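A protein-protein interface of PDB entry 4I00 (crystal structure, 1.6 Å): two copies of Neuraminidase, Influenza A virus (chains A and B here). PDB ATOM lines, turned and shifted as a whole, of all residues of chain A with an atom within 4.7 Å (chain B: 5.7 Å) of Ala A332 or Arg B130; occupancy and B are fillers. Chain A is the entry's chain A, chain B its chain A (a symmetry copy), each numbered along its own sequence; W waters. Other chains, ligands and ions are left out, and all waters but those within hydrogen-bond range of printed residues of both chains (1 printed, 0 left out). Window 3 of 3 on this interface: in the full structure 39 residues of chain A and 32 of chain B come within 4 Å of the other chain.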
ATOM      1  N   CYS A  11     -28.902 -23.597 -12.991  1.00  0.00           N
ATOM      2  CA  CYS A  11     -29.997 -23.067 -12.179  1.00  0.00           C
ATOM      3  C   CYS A  11     -31.236 -22.836 -13.032  1.00  0.00           C
ATOM      4  O   CYS A  11     -31.137 -22.587 -14.223  1.00  0.00           O
ATOM      5  CB  CYS A  11     -29.598 -21.732 -11.542  1.00  0.00           C
ATOM      6  SG  CYS A  11     -28.142 -21.768 -10.488  1.00  0.00           S
ATOM      7  N   VAL A 330     -21.826 -18.683 -13.409  1.00  0.00           N
ATOM      8  CA  VAL A 330     -21.448 -18.228 -12.079  1.00  0.00           C
ATOM      9  C   VAL A 330     -22.000 -19.206 -11.054  1.00  0.00           C
ATOM     10  O   VAL A 330     -23.177 -19.545 -11.103  1.00  0.00           O
ATOM     11  CB  VAL A 330     -21.996 -16.819 -11.779  1.00  0.00           C
ATOM     12  CG1 VAL A 330     -21.518 -16.362 -10.414  1.00  0.00           C
ATOM     13  CG2 VAL A 330     -21.564 -15.839 -12.864  1.00  0.00           C
ATOM     14  N   LYS A 331     -21.165 -19.687 -10.142  1.00  0.00           N
ATOM     15  CA  LYS A 331     -21.653 -20.659  -9.174  1.00  0.00           C
ATOM     16  C   LYS A 331     -22.658 -20.025  -8.210  1.00  0.00           C
ATOM     17  O   LYS A 331     -22.393 -18.976  -7.629  1.00  0.00           O
ATOM     18  CB  LYS A 331     -20.515 -21.299  -8.390  1.00  0.00           C
ATOM     19  CG  LYS A 331     -20.984 -22.452  -7.521  1.00  0.00           C
ATOM     20  CD  LYS A 331     -19.839 -23.096  -6.760  1.00  0.00           C
ATOM     21  CE  LYS A 331     -20.363 -24.242  -5.900  1.00  0.00           C
ATOM     22  NZ  LYS A 331     -20.011 -24.083  -4.463  1.00  0.00           N
ATOM     23  N   ALA A 332     -23.807 -20.647  -8.085  1.00  0.00           N
ATOM     24  CA  ALA A 332     -24.768 -20.194  -7.166  1.00  0.00           C
ATOM     25  C   ALA A 332     -24.651 -21.172  -6.008  1.00  0.00           C
ATOM     26  O   ALA A 332     -23.583 -21.361  -5.536  1.00  0.00           O
ATOM     27  CB  ALA A 332     -26.066 -20.103  -7.766  1.00  0.00           C
ATOM     28  N   LYS A 333     -25.634 -21.782  -5.461  1.00  0.00           N
ATOM     29  CA  LYS A 333     -25.133 -22.537  -4.322  1.00  0.00           C
ATOM     30  C   LYS A 333     -24.772 -23.944  -4.726  1.00  0.00           C
ATOM     31  O   LYS A 333     -23.675 -24.414  -4.665  1.00  0.00           O
ATOM     32  CB  LYS A 333     -26.124 -22.556  -3.192  1.00  0.00           C
ATOM     33  CG  LYS A 333     -26.585 -21.231  -2.865  1.00  0.00           C
ATOM     34  CD  LYS A 333     -25.730 -20.612  -1.803  1.00  0.00           C
ATOM     35  CE  LYS A 333     -26.608 -20.017  -0.747  1.00  0.00           C
ATOM     36  NZ  LYS A 333     -25.758 -19.293   0.151  1.00  0.00           N
ATOM     37  N   ASP A 334     -25.786 -24.554  -5.193  1.00  0.00           N
ATOM     38  CA  ASP A 334     -25.751 -25.913  -5.725  1.00  0.00           C
ATOM     39  C   ASP A 334     -26.178 -25.981  -7.191  1.00  0.00           C
ATOM     40  O   ASP A 334     -26.607 -27.024  -7.676  1.00  0.00           O
ATOM     41  CB  ASP A 334     -26.602 -26.845  -4.860  1.00  0.00           C
ATOM     42  CG  ASP A 334     -27.912 -26.213  -4.444  1.00  0.00           C
ATOM     43  OD1 ASP A 334     -28.330 -26.421  -3.281  1.00  0.00           O
ATOM     44  OD2 ASP A 334     -28.517 -25.496  -5.274  1.00  0.00           O
ATOM     45  N   CYS A 335     -26.057 -24.863  -7.894  1.00  0.00           N
ATOM     46  CA  CYS A 335     -26.296 -24.838  -9.333  1.00  0.00           C
ATOM     47  C   CYS A 335     -25.449 -23.744  -9.976  1.00  0.00           C
ATOM     48  O   CYS A 335     -24.931 -22.869  -9.285  1.00  0.00           O
ATOM     49  CB  CYS A 335     -27.788 -24.677  -9.674  1.00  0.00           C
ATOM     50  SG  CYS A 335     -28.590 -23.148  -9.061  1.00  0.00           S
ATOM     51  N   PHE A 336     -25.291 -23.816 -11.292  1.00  0.00           N
ATOM     52  CA  PHE A 336     -24.567 -22.793 -12.032  1.00  0.00           C
ATOM     53  C   PHE A 336     -25.562 -21.874 -12.716  1.00  0.00           C
ATOM     54  O   PHE A 336     -26.494 -22.333 -13.368  1.00  0.00           O
ATOM     55  CB  PHE A 336     -23.680 -23.419 -13.107  1.00  0.00           C
ATOM     56  CG  PHE A 336     -22.441 -24.062 -12.575  1.00  0.00           C
ATOM     57  CD1 PHE A 336     -21.527 -23.334 -11.830  1.00  0.00           C
ATOM     58  CD2 PHE A 336     -22.159 -25.389 -12.858  1.00  0.00           C
ATOM     59  CE1 PHE A 336     -20.367 -23.927 -11.345  1.00  0.00           C
ATOM     60  CE2 PHE A 336     -20.998 -25.989 -12.384  1.00  0.00           C
ATOM     61  CZ  PHE A 336     -20.098 -25.257 -11.624  1.00  0.00           C
ATOM     62  N   GLN A 337     -25.367 -20.571 -12.569  1.00  0.00           N
ATOM     63  CA  GLN A 337     -26.249 -19.610 -13.206  1.00  0.00           C
ATOM     64  C   GLN A 337     -25.764 -19.329 -14.626  1.00  0.00           C
ATOM     65  O   GLN A 337     -24.573 -19.086 -14.839  1.00  0.00           O
ATOM     66  CB  GLN A 337     -26.256 -18.329 -12.375  1.00  0.00           C
ATOM     67  CG  GLN A 337     -26.986 -17.167 -13.007  1.00  0.00           C
ATOM     68  CD  GLN A 337     -26.831 -15.916 -12.176  1.00  0.00           C
ATOM     69  OE1 GLN A 337     -25.779 -15.686 -11.574  1.00  0.00           O
ATOM     70  NE2 GLN A 337     -27.879 -15.104 -12.122  1.00  0.00           N
ATOM     71  N   ILE B 125     -30.519  -7.478  -8.139  1.00  0.00           N
ATOM     72  CA  ILE B 125     -29.885  -7.642  -6.839  1.00  0.00           C
ATOM     73  C   ILE B 125     -28.579  -8.399  -7.014  1.00  0.00           C
ATOM     74  O   ILE B 125     -28.572  -9.506  -7.534  1.00  0.00           O
ATOM     75  CB  ILE B 125     -30.783  -8.421  -5.854  1.00  0.00           C
ATOM     76  CG1 ILE B 125     -32.207  -7.854  -5.870  1.00  0.00           C
ATOM     77  CG2 ILE B 125     -30.180  -8.413  -4.448  1.00  0.00           C
ATOM     78  CD1 ILE B 125     -32.315  -6.427  -5.313  1.00  0.00           C
ATOM     79  N   ILE B 126     -27.479  -7.768  -6.617  1.00  0.00           N
ATOM     80  CA  ILE B 126     -26.160  -8.384  -6.654  1.00  0.00           C
ATOM     81  C   ILE B 126     -25.730  -8.698  -5.223  1.00  0.00           C
ATOM     82  O   ILE B 126     -25.871  -7.865  -4.325  1.00  0.00           O
ATOM     83  CB  ILE B 126     -25.092  -7.438  -7.273  1.00  0.00           C
ATOM     84  CG1 ILE B 126     -25.622  -6.727  -8.524  1.00  0.00           C
ATOM     85  CG2 ILE B 126     -23.785  -8.203  -7.555  1.00  0.00           C
ATOM     86  CD1 ILE B 126     -26.111  -7.642  -9.597  1.00  0.00           C
ATOM     87  N   TYR B 127     -25.213  -9.906  -5.011  1.00  0.00           N
ATOM     88  CA  TYR B 127     -24.706 -10.290  -3.701  1.00  0.00           C
ATOM     89  C   TYR B 127     -23.408 -11.076  -3.851  1.00  0.00           C
ATOM     90  O   TYR B 127     -23.374 -12.136  -4.464  1.00  0.00           O
ATOM     91  CB  TYR B 127     -25.732 -11.101  -2.910  1.00  0.00           C
ATOM     92  CG  TYR B 127     -25.276 -11.405  -1.495  1.00  0.00           C
ATOM     93  CD1 TYR B 127     -25.379 -10.446  -0.493  1.00  0.00           C
ATOM     94  CD2 TYR B 127     -24.739 -12.647  -1.166  1.00  0.00           C
ATOM     95  CE1 TYR B 127     -24.958 -10.712   0.814  1.00  0.00           C
ATOM     96  CE2 TYR B 127     -24.321 -12.921   0.128  1.00  0.00           C
ATOM     97  CZ  TYR B 127     -24.440 -11.953   1.118  1.00  0.00           C
ATOM     98  OH  TYR B 127     -24.017 -12.231   2.400  1.00  0.00           O
ATOM     99  N   GLY B 128     -22.336 -10.551  -3.268  1.00  0.00           N
ATOM    100  CA  GLY B 128     -21.033 -11.195  -3.422  1.00  0.00           C
ATOM    101  C   GLY B 128     -20.619 -11.288  -4.882  1.00  0.00           C
ATOM    102  O   GLY B 128     -19.908 -12.221  -5.295  1.00  0.00           O
ATOM    103  N   GLY B 129     -21.073 -10.325  -5.676  1.00  0.00           N
ATOM    104  CA  GLY B 129     -20.670 -10.238  -7.068  1.00  0.00           C
ATOM    105  C   GLY B 129     -21.582 -10.999  -8.020  1.00  0.00           C
ATOM    106  O   GLY B 129     -21.444 -10.863  -9.240  1.00  0.00           O
ATOM    107  N   ARG B 130     -22.491 -11.808  -7.479  1.00  0.00           N
ATOM    108  CA  ARG B 130     -23.393 -12.605  -8.305  1.00  0.00           C
ATOM    109  C   ARG B 130     -24.772 -11.976  -8.366  1.00  0.00           C
ATOM    110  O   ARG B 130     -25.288 -11.528  -7.357  1.00  0.00           O
ATOM    111  CB  ARG B 130     -23.524 -14.026  -7.750  1.00  0.00           C
ATOM    112  CG  ARG B 130     -24.291 -14.961  -8.681  1.00  0.00           C
ATOM    113  CD  ARG B 130     -24.339 -16.382  -8.156  1.00  0.00           C
ATOM    114  NE  ARG B 130     -25.624 -16.719  -7.565  1.00  0.00           N
ATOM    115  CZ  ARG B 130     -25.862 -16.820  -6.263  1.00  0.00           C
ATOM    116  NH1 ARG B 130     -24.896 -16.593  -5.367  1.00  0.00           N
ATOM    117  NH2 ARG B 130     -27.085 -17.148  -5.855  1.00  0.00           N
ATOM    118  N   MET B 131     -25.371 -11.936  -9.544  1.00  0.00           N
ATOM    119  CA  MET B 131     -26.769 -11.514  -9.625  1.00  0.00           C
ATOM    120  C   MET B 131     -27.669 -12.602  -9.037  1.00  0.00           C
ATOM    121  O   MET B 131     -27.756 -13.699  -9.585  1.00  0.00           O
ATOM    122  CB  MET B 131     -27.172 -11.239 -11.067  1.00  0.00           C
ATOM    123  CG  MET B 131     -28.586 -10.639 -11.160  1.00  0.00           C
ATOM    124  SD  MET B 131     -29.112 -10.423 -12.865  1.00  0.00           S
ATOM    125  CE  MET B 131     -27.814  -9.329 -13.462  1.00  0.00           C
ATOM    126  N   THR B 132     -28.331 -12.294  -7.926  1.00  0.00           N
ATOM    127  CA  THR B 132     -29.086 -13.282  -7.154  1.00  0.00           C
ATOM    128  C   THR B 132     -30.611 -13.141  -7.213  1.00  0.00           C
ATOM    129  O   THR B 132     -31.329 -14.086  -6.889  1.00  0.00           O
ATOM    130  CB  THR B 132     -28.717 -13.205  -5.673  1.00  0.00           C
ATOM    131  OG1 THR B 132     -28.766 -11.836  -5.248  1.00  0.00           O
ATOM    132  CG2 THR B 132     -27.317 -13.737  -5.431  1.00  0.00           C
ATOM    133  N   LYS B 181     -31.219 -12.735  -1.666  1.00  0.00           N
ATOM    134  CA  LYS B 181     -32.554 -13.244  -1.993  1.00  0.00           C
ATOM    135  C   LYS B 181     -33.647 -12.438  -1.311  1.00  0.00           C
ATOM    136  O   LYS B 181     -33.631 -12.255  -0.094  1.00  0.00           O
ATOM    137  CB  LYS B 181     -32.674 -14.723  -1.628  1.00  0.00           C
ATOM    138  CG  LYS B 181     -31.699 -15.617  -2.388  1.00  0.00           C
ATOM    139  CD  LYS B 181     -31.798 -15.395  -3.908  1.00  0.00           C
ATOM    140  CE  LYS B 181     -30.885 -16.327  -4.685  1.00  0.00           C
ATOM    141  NZ  LYS B 181     -31.557 -17.619  -5.025  1.00  0.00           N
HETATM  142  O   HOH W   1     -24.293 -13.362 -11.727  1.00  0.00           O
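NE2 of Gln A337 sits at hydrogen-bond distance from O of Met B131 (2.9 Å).
The side-chain sulfur (SG) of Cys A11 lies within hydrogen-bond range of the backbone NH (N) of Gln A337 (3.7 Å). The backbone carbonyl oxygen of Val A330 lies within hydrogen-bond range of the backbone NH of Gln A337, 2.8 Å away. SG of Cys A11 is disulfide-bonded to SG of Cys A335 (2.0 Å).
Among the printed residues, merely in contact across the chains: Val A330 with Arg B130 (3.6 Å), Lys A331 with Arg B130 (3.3 Å), Ala A332 with Arg B130 (3.4 Å) and Gln A337 with Arg B130 (3.3 Å).
Ala A332 touches just one residue of chain B: Arg B130 (3.4 Å). Of the printed residues of chain A, Arg B130 touches Val A330 (3.6 Å), Lys A331 (3.3 Å), Ala A332 (3.4 Å) and Gln A337 (3.3 Å). Printed residues of chain B within 4 Å of Gln A337: Arg B130 and Met B131. Of the printed residues of chain A, Met B131 touches Gln A337 (2.9 Å). Of the printed residues of chain B, Lys A331 touches Arg B130 (3.3 Å). Of the printed residues of chain B, Val A330 touches Arg B130 (3.6 Å). Lys A333 touches none of the printed residues of chain B. Gly B129 touches none of the printed residues of chain A. The nearest printed residue of chain A that does not touch Arg B130 is Lys A333 (4.9 Å).
Of the 9 printed residues of chain A, 4 touch a printed residue of chain B. Hydrophobic or aromatic side chains of chain A within 4 Å of the printed part of chain B: Val A330 and Ala A332. Among the printed residues, 5 pairs touch across the chains. Among the printed residues, no Asp or Glu carboxylate lies within 4 Å of a Lys or Arg side-chain nitrogen of the other chain.
No position is printed for both chains.
Water W1 lies within hydrogen-bond range of the side-chain amide oxygen (OE1) of Gln A337 and the backbone NH (N) of Met B131.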
